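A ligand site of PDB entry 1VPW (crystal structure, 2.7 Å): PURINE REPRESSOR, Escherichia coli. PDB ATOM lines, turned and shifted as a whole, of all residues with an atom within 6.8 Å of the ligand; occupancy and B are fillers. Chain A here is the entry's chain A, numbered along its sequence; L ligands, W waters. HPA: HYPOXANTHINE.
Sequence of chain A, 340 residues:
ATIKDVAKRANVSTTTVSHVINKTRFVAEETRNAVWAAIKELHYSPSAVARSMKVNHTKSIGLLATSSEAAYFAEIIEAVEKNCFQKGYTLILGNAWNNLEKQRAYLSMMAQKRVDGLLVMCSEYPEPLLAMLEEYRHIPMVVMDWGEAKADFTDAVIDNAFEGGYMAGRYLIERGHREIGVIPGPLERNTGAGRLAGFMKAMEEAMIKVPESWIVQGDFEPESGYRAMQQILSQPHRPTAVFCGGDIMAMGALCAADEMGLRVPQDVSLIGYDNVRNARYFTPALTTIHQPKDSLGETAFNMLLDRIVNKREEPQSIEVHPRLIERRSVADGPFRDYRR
NH2 of Arg 189 sits at hydrogen-bond distance from O6 of the ligand (2.7 Å). OD2 of Asp 274 lies close to N9 of the ligand, 2.9 Å away. The side-chain hydroxyl of Thr 191 is in hydrogen-bond range of a nitrogen (N7) of the ligand.
Residues that only touch the ligand: Tyr 72 (3.1 Å), Phe 73 (3.3 Å), Arg 195 (3.5 Å) and Phe 220 (3.3 Å). Hydrophobic or aromatic side chains within 4 Å of the ligand: Tyr 72, Phe 73 and Phe 220. Of the 23 residues printed, 7 come within 4 Å of the ligand. The nearest printed residue that does not touch the ligand is Ser 123 (4.01 Å).
Water W1 lies within hydrogen-bond range of N3 of the ligand (3.1 Å) and N of Tyr 72 (3.1 Å). Water W2 lies within hydrogen-bond range of the guanidinium group (NH2) of Arg 189 (2.7 Å) and a nitrogen (N1) of the ligand (3.1 Å).
The backbone carbonyl oxygen (O) of Asp 274 sits at hydrogen-bond distance from the backbone NH (N) of Gln 291 (3.2 Å). The backbone carbonyl oxygen (O) of Gly 245 sits at hydrogen-bond distance from the guanidinium group (NH1) of Arg 195, at 2.8 Å. OD1 of Asp 274 is in salt-bridge range of NH2 of Arg 195 (2.6 Å). The side-chain hydroxyl (OH) of Tyr 72 lies within hydrogen-bond range of the side-chain amide oxygen (OE1) of Gln 291, 2.8 Å away.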
ATOM      1  N   THR A  66       9.299  18.292 -15.466  1.00  0.00           N
ATOM      2  CA  THR A  66       9.612  18.327 -14.041  1.00  0.00           C
ATOM      3  C   THR A  66       8.779  19.417 -13.354  1.00  0.00           C
ATOM      4  O   THR A  66       8.069  19.175 -12.377  1.00  0.00           O
ATOM      5  CB  THR A  66      11.046  18.656 -13.832  1.00  0.00           C
ATOM      6  OG1 THR A  66      11.871  17.550 -14.253  1.00  0.00           O
ATOM      7  CG2 THR A  66      11.282  18.946 -12.382  1.00  0.00           C
ATOM      8  N   SER A  67       8.862  20.636 -13.882  1.00  0.00           N
ATOM      9  CA  SER A  67       8.114  21.766 -13.346  1.00  0.00           C
ATOM     10  C   SER A  67       8.076  22.822 -14.439  1.00  0.00           C
ATOM     11  O   SER A  67       8.867  22.787 -15.387  1.00  0.00           O
ATOM     12  CB  SER A  67       8.776  22.294 -12.042  1.00  0.00           C
ATOM     13  OG  SER A  67       9.429  23.556 -12.217  1.00  0.00           O
ATOM     14  N   ALA A  70      10.018  27.513 -13.164  1.00  0.00           N
ATOM     15  CA  ALA A  70      11.438  27.773 -13.367  1.00  0.00           C
ATOM     16  C   ALA A  70      11.786  28.293 -14.783  1.00  0.00           C
ATOM     17  O   ALA A  70      11.589  27.610 -15.793  1.00  0.00           O
ATOM     18  CB  ALA A  70      12.223  26.526 -13.067  1.00  0.00           C
ATOM     19  N   ALA A  71      12.318  29.518 -14.807  1.00  0.00           N
ATOM     20  CA  ALA A  71      12.725  30.200 -16.035  1.00  0.00           C
ATOM     21  C   ALA A  71      13.267  29.262 -17.089  1.00  0.00           C
ATOM     22  O   ALA A  71      12.733  29.174 -18.200  1.00  0.00           O
ATOM     23  CB  ALA A  71      13.767  31.239 -15.706  1.00  0.00           C
ATOM     24  N   TYR A  72      14.342  28.574 -16.725  1.00  0.00           N
ATOM     25  CA  TYR A  72      14.994  27.651 -17.628  1.00  0.00           C
ATOM     26  C   TYR A  72      13.896  26.824 -18.295  1.00  0.00           C
ATOM     27  O   TYR A  72      13.586  26.979 -19.463  1.00  0.00           O
ATOM     28  CB  TYR A  72      15.922  26.771 -16.811  1.00  0.00           C
ATOM     29  CG  TYR A  72      16.652  25.751 -17.602  1.00  0.00           C
ATOM     30  CD1 TYR A  72      17.656  26.120 -18.454  1.00  0.00           C
ATOM     31  CD2 TYR A  72      16.324  24.418 -17.498  1.00  0.00           C
ATOM     32  CE1 TYR A  72      18.340  25.176 -19.197  1.00  0.00           C
ATOM     33  CE2 TYR A  72      17.013  23.467 -18.237  1.00  0.00           C
ATOM     34  CZ  TYR A  72      18.007  23.857 -19.085  1.00  0.00           C
ATOM     35  OH  TYR A  72      18.683  22.949 -19.825  1.00  0.00           O
ATOM     36  N   PHE A  73      13.218  26.058 -17.476  1.00  0.00           N
ATOM     37  CA  PHE A  73      12.132  25.241 -17.928  1.00  0.00           C
ATOM     38  C   PHE A  73      11.113  25.944 -18.758  1.00  0.00           C
ATOM     39  O   PHE A  73      10.754  25.522 -19.842  1.00  0.00           O
ATOM     40  CB  PHE A  73      11.455  24.652 -16.728  1.00  0.00           C
ATOM     41  CG  PHE A  73      12.260  23.595 -16.072  1.00  0.00           C
ATOM     42  CD1 PHE A  73      13.137  22.819 -16.826  1.00  0.00           C
ATOM     43  CD2 PHE A  73      12.163  23.365 -14.709  1.00  0.00           C
ATOM     44  CE1 PHE A  73      13.887  21.858 -16.241  1.00  0.00           C
ATOM     45  CE2 PHE A  73      12.916  22.375 -14.132  1.00  0.00           C
ATOM     46  CZ  PHE A  73      13.784  21.628 -14.894  1.00  0.00           C
ATOM     47  N   SER A 123      14.635  15.612 -15.467  1.00  0.00           N
ATOM     48  CA  SER A 123      15.738  16.038 -14.617  1.00  0.00           C
ATOM     49  C   SER A 123      16.505  14.875 -14.102  1.00  0.00           C
ATOM     50  O   SER A 123      17.627  14.688 -14.469  1.00  0.00           O
ATOM     51  CB  SER A 123      15.259  16.908 -13.450  1.00  0.00           C
ATOM     52  OG  SER A 123      14.541  18.039 -13.915  1.00  0.00           O
ATOM     53  N   PRO A 186      22.035  20.091  -8.517  1.00  0.00           N
ATOM     54  CA  PRO A 186      21.907  18.682  -8.153  1.00  0.00           C
ATOM     55  C   PRO A 186      22.728  17.767  -9.035  1.00  0.00           C
ATOM     56  O   PRO A 186      22.622  17.797 -10.244  1.00  0.00           O
ATOM     57  CB  PRO A 186      20.431  18.406  -8.358  1.00  0.00           C
ATOM     58  CG  PRO A 186      19.776  19.773  -8.415  1.00  0.00           C
ATOM     59  CD  PRO A 186      20.781  20.650  -9.035  1.00  0.00           C
ATOM     60  N   ARG A 189      21.458  15.362 -11.794  1.00  0.00           N
ATOM     61  CA  ARG A 189      21.016  15.945 -13.064  1.00  0.00           C
ATOM     62  C   ARG A 189      22.194  16.248 -13.958  1.00  0.00           C
ATOM     63  O   ARG A 189      23.312  16.481 -13.488  1.00  0.00           O
ATOM     64  CB  ARG A 189      20.200  17.203 -12.858  1.00  0.00           C
ATOM     65  CG  ARG A 189      18.797  16.937 -12.545  1.00  0.00           C
ATOM     66  CD  ARG A 189      18.415  17.644 -11.334  1.00  0.00           C
ATOM     67  NE  ARG A 189      17.701  18.848 -11.678  1.00  0.00           N
ATOM     68  CZ  ARG A 189      16.581  19.202 -11.089  1.00  0.00           C
ATOM     69  NH1 ARG A 189      16.092  18.429 -10.159  1.00  0.00           N
ATOM     70  NH2 ARG A 189      15.942  20.328 -11.423  1.00  0.00           N
ATOM     71  N   ASN A 190      21.941  16.246 -15.258  1.00  0.00           N
ATOM     72  CA  ASN A 190      22.978  16.517 -16.226  1.00  0.00           C
ATOM     73  C   ASN A 190      23.532  17.936 -16.029  1.00  0.00           C
ATOM     74  O   ASN A 190      24.745  18.114 -15.794  1.00  0.00           O
ATOM     75  CB  ASN A 190      22.432  16.326 -17.646  1.00  0.00           C
ATOM     76  CG  ASN A 190      23.457  16.589 -18.683  1.00  0.00           C
ATOM     77  OD1 ASN A 190      24.570  16.049 -18.623  1.00  0.00           O
ATOM     78  ND2 ASN A 190      23.158  17.579 -19.552  1.00  0.00           N
ATOM     79  N   THR A 191      22.643  18.932 -16.124  1.00  0.00           N
ATOM     80  CA  THR A 191      22.998  20.332 -15.956  1.00  0.00           C
ATOM     81  C   THR A 191      23.710  20.558 -14.630  1.00  0.00           C
ATOM     82  O   THR A 191      24.353  21.600 -14.426  1.00  0.00           O
ATOM     83  CB  THR A 191      21.765  21.230 -16.019  1.00  0.00           C
ATOM     84  OG1 THR A 191      20.765  20.706 -15.140  1.00  0.00           O
ATOM     85  CG2 THR A 191      21.205  21.295 -17.444  1.00  0.00           C
ATOM     86  N   GLY A 192      23.604  19.575 -13.731  1.00  0.00           N
ATOM     87  CA  GLY A 192      24.255  19.621 -12.434  1.00  0.00           C
ATOM     88  C   GLY A 192      25.660  19.031 -12.556  1.00  0.00           C
ATOM     89  O   GLY A 192      26.612  19.711 -12.891  1.00  0.00           O
ATOM     90  N   ARG A 195      27.850  19.969 -15.683  1.00  0.00           N
ATOM     91  CA  ARG A 195      28.420  21.288 -15.823  1.00  0.00           C
ATOM     92  C   ARG A 195      29.604  21.375 -14.863  1.00  0.00           C
ATOM     93  O   ARG A 195      30.666  21.918 -15.195  1.00  0.00           O
ATOM     94  CB  ARG A 195      27.363  22.376 -15.553  1.00  0.00           C
ATOM     95  CG  ARG A 195      26.284  22.546 -16.680  1.00  0.00           C
ATOM     96  CD  ARG A 195      25.141  23.516 -16.302  1.00  0.00           C
ATOM     97  NE  ARG A 195      24.078  23.616 -17.313  1.00  0.00           N
ATOM     98  CZ  ARG A 195      23.031  24.465 -17.240  1.00  0.00           C
ATOM     99  NH1 ARG A 195      22.922  25.309 -16.214  1.00  0.00           N
ATOM    100  NH2 ARG A 195      22.098  24.464 -18.187  1.00  0.00           N
ATOM    101  N   ASP A 219      20.138  23.963  -5.753  1.00  0.00           N
ATOM    102  CA  ASP A 219      19.063  23.137  -6.258  1.00  0.00           C
ATOM    103  C   ASP A 219      18.422  23.837  -7.458  1.00  0.00           C
ATOM    104  O   ASP A 219      17.318  23.497  -7.873  1.00  0.00           O
ATOM    105  CB  ASP A 219      18.045  22.902  -5.131  1.00  0.00           C
ATOM    106  CG  ASP A 219      17.507  24.186  -4.557  1.00  0.00           C
ATOM    107  OD1 ASP A 219      17.398  25.176  -5.302  1.00  0.00           O
ATOM    108  OD2 ASP A 219      17.105  24.177  -3.378  1.00  0.00           O
ATOM    109  N   PHE A 220      19.119  24.848  -7.963  1.00  0.00           N
ATOM    110  CA  PHE A 220      18.676  25.696  -9.095  1.00  0.00           C
ATOM    111  C   PHE A 220      17.743  26.818  -8.678  1.00  0.00           C
ATOM    112  O   PHE A 220      17.361  27.653  -9.483  1.00  0.00           O
ATOM    113  CB  PHE A 220      18.024  24.886 -10.222  1.00  0.00           C
ATOM    114  CG  PHE A 220      19.009  24.149 -11.062  1.00  0.00           C
ATOM    115  CD1 PHE A 220      20.021  24.833 -11.699  1.00  0.00           C
ATOM    116  CD2 PHE A 220      18.957  22.775 -11.152  1.00  0.00           C
ATOM    117  CE1 PHE A 220      20.954  24.159 -12.433  1.00  0.00           C
ATOM    118  CE2 PHE A 220      19.872  22.096 -11.874  1.00  0.00           C
ATOM    119  CZ  PHE A 220      20.879  22.794 -12.527  1.00  0.00           C
ATOM    120  N   GLU A 221      17.372  26.844  -7.407  1.00  0.00           N
ATOM    121  CA  GLU A 221      16.492  27.907  -6.924  1.00  0.00           C
ATOM    122  C   GLU A 221      17.266  29.025  -6.201  1.00  0.00           C
ATOM    123  O   GLU A 221      18.224  28.766  -5.437  1.00  0.00           O
ATOM    124  CB  GLU A 221      15.378  27.342  -6.073  1.00  0.00           C
ATOM    125  CG  GLU A 221      14.509  26.330  -6.822  1.00  0.00           C
ATOM    126  CD  GLU A 221      13.267  26.943  -7.423  1.00  0.00           C
ATOM    127  OE1 GLU A 221      13.364  27.604  -8.476  1.00  0.00           O
ATOM    128  OE2 GLU A 221      12.185  26.732  -6.836  1.00  0.00           O
ATOM    129  N   GLY A 245      26.300  27.250 -11.118  1.00  0.00           N
ATOM    130  CA  GLY A 245      25.590  26.266 -11.965  1.00  0.00           C
ATOM    131  C   GLY A 245      24.352  26.704 -12.783  1.00  0.00           C
ATOM    132  O   GLY A 245      24.007  26.049 -13.752  1.00  0.00           O
ATOM    133  N   GLY A 246      23.680  27.769 -12.385  1.00  0.00           N
ATOM    134  CA  GLY A 246      22.480  28.255 -13.093  1.00  0.00           C
ATOM    135  C   GLY A 246      22.189  29.768 -12.840  1.00  0.00           C
ATOM    136  O   GLY A 246      22.462  30.324 -11.767  1.00  0.00           O
ATOM    137  N   ASP A 247      21.603  30.439 -13.827  1.00  0.00           N
ATOM    138  CA  ASP A 247      21.315  31.843 -13.674  1.00  0.00           C
ATOM    139  C   ASP A 247      20.445  32.257 -12.456  1.00  0.00           C
ATOM    140  O   ASP A 247      20.790  33.179 -11.679  1.00  0.00           O
ATOM    141  CB  ASP A 247      20.798  32.417 -14.961  1.00  0.00           C
ATOM    142  CG  ASP A 247      21.868  32.449 -16.059  1.00  0.00           C
ATOM    143  OD1 ASP A 247      23.021  32.065 -15.773  1.00  0.00           O
ATOM    144  OD2 ASP A 247      21.557  32.945 -17.168  1.00  0.00           O
ATOM    145  N   ILE A 248      19.305  31.597 -12.306  1.00  0.00           N
ATOM    146  CA  ILE A 248      18.421  31.911 -11.201  1.00  0.00           C
ATOM    147  C   ILE A 248      19.102  31.779  -9.832  1.00  0.00           C
ATOM    148  O   ILE A 248      18.930  32.611  -8.962  1.00  0.00           O
ATOM    149  CB  ILE A 248      17.119  31.112 -11.266  1.00  0.00           C
ATOM    150  CG1 ILE A 248      16.433  31.324 -12.608  1.00  0.00           C
ATOM    151  CG2 ILE A 248      16.194  31.494 -10.134  1.00  0.00           C
ATOM    152  CD1 ILE A 248      16.128  32.700 -12.908  1.00  0.00           C
ATOM    153  N   TYR A 273      25.130  30.365 -15.565  1.00  0.00           N
ATOM    154  CA  TYR A 273      24.927  29.398 -16.618  1.00  0.00           C
ATOM    155  C   TYR A 273      23.471  29.210 -16.928  1.00  0.00           C
ATOM    156  O   TYR A 273      22.700  28.866 -16.035  1.00  0.00           O
ATOM    157  CB  TYR A 273      25.455  28.062 -16.163  1.00  0.00           C
ATOM    158  CG  TYR A 273      25.730  27.125 -17.296  1.00  0.00           C
ATOM    159  CD1 TYR A 273      24.831  26.976 -18.331  1.00  0.00           C
ATOM    160  CD2 TYR A 273      26.902  26.386 -17.327  1.00  0.00           C
ATOM    161  CE1 TYR A 273      25.101  26.112 -19.375  1.00  0.00           C
ATOM    162  CE2 TYR A 273      27.183  25.528 -18.351  1.00  0.00           C
ATOM    163  CZ  TYR A 273      26.291  25.386 -19.381  1.00  0.00           C
ATOM    164  OH  TYR A 273      26.588  24.505 -20.417  1.00  0.00           O
ATOM    165  N   ASP A 274      23.147  29.400 -18.207  1.00  0.00           N
ATOM    166  CA  ASP A 274      21.796  29.212 -18.810  1.00  0.00           C
ATOM    167  C   ASP A 274      21.496  30.327 -19.787  1.00  0.00           C
ATOM    168  O   ASP A 274      20.906  30.124 -20.843  1.00  0.00           O
ATOM    169  CB  ASP A 274      20.674  29.170 -17.760  1.00  0.00           C
ATOM    170  CG  ASP A 274      20.442  27.773 -17.177  1.00  0.00           C
ATOM    171  OD1 ASP A 274      21.070  26.803 -17.663  1.00  0.00           O
ATOM    172  OD2 ASP A 274      19.691  27.670 -16.166  1.00  0.00           O
ATOM    173  N   GLN A 291      22.640  28.611 -23.058  1.00  0.00           N
ATOM    174  CA  GLN A 291      22.175  27.322 -23.535  1.00  0.00           C
ATOM    175  C   GLN A 291      21.099  27.623 -24.508  1.00  0.00           C
ATOM    176  O   GLN A 291      20.161  28.339 -24.187  1.00  0.00           O
ATOM    177  CB  GLN A 291      21.531  26.502 -22.428  1.00  0.00           C
ATOM    178  CG  GLN A 291      20.818  25.225 -22.960  1.00  0.00           C
ATOM    179  CD  GLN A 291      21.460  23.953 -22.415  1.00  0.00           C
ATOM    180  OE1 GLN A 291      20.913  23.305 -21.524  1.00  0.00           O
ATOM    181  NE2 GLN A 291      22.710  23.698 -22.821  1.00  0.00           N
HETATM  182  N1  HPA L   1      16.141  23.106 -13.122  1.00  0.00           N
HETATM  183  C2  HPA L   1      16.043  24.476 -13.213  1.00  0.00           C
HETATM  184  N3  HPA L   1      16.842  25.247 -13.934  1.00  0.00           N
HETATM  185  C4  HPA L   1      17.782  24.524 -14.598  1.00  0.00           C
HETATM  186  C5  HPA L   1      17.962  23.161 -14.573  1.00  0.00           C
HETATM  187  C6  HPA L   1      17.095  22.346 -13.798  1.00  0.00           C
HETATM  188  O6  HPA L   1      17.100  21.120 -13.674  1.00  0.00           O
HETATM  189  N7  HPA L   1      19.026  22.800 -15.386  1.00  0.00           N
HETATM  190  C8  HPA L   1      19.460  23.933 -15.878  1.00  0.00           C
HETATM  191  N9  HPA L   1      18.733  25.017 -15.448  1.00  0.00           N
HETATM  192  O   HOH W   1      15.763  28.106 -13.966  1.00  0.00           O
HETATM  193  O   HOH W   2      14.434  22.493 -10.648  1.00  0.00           O
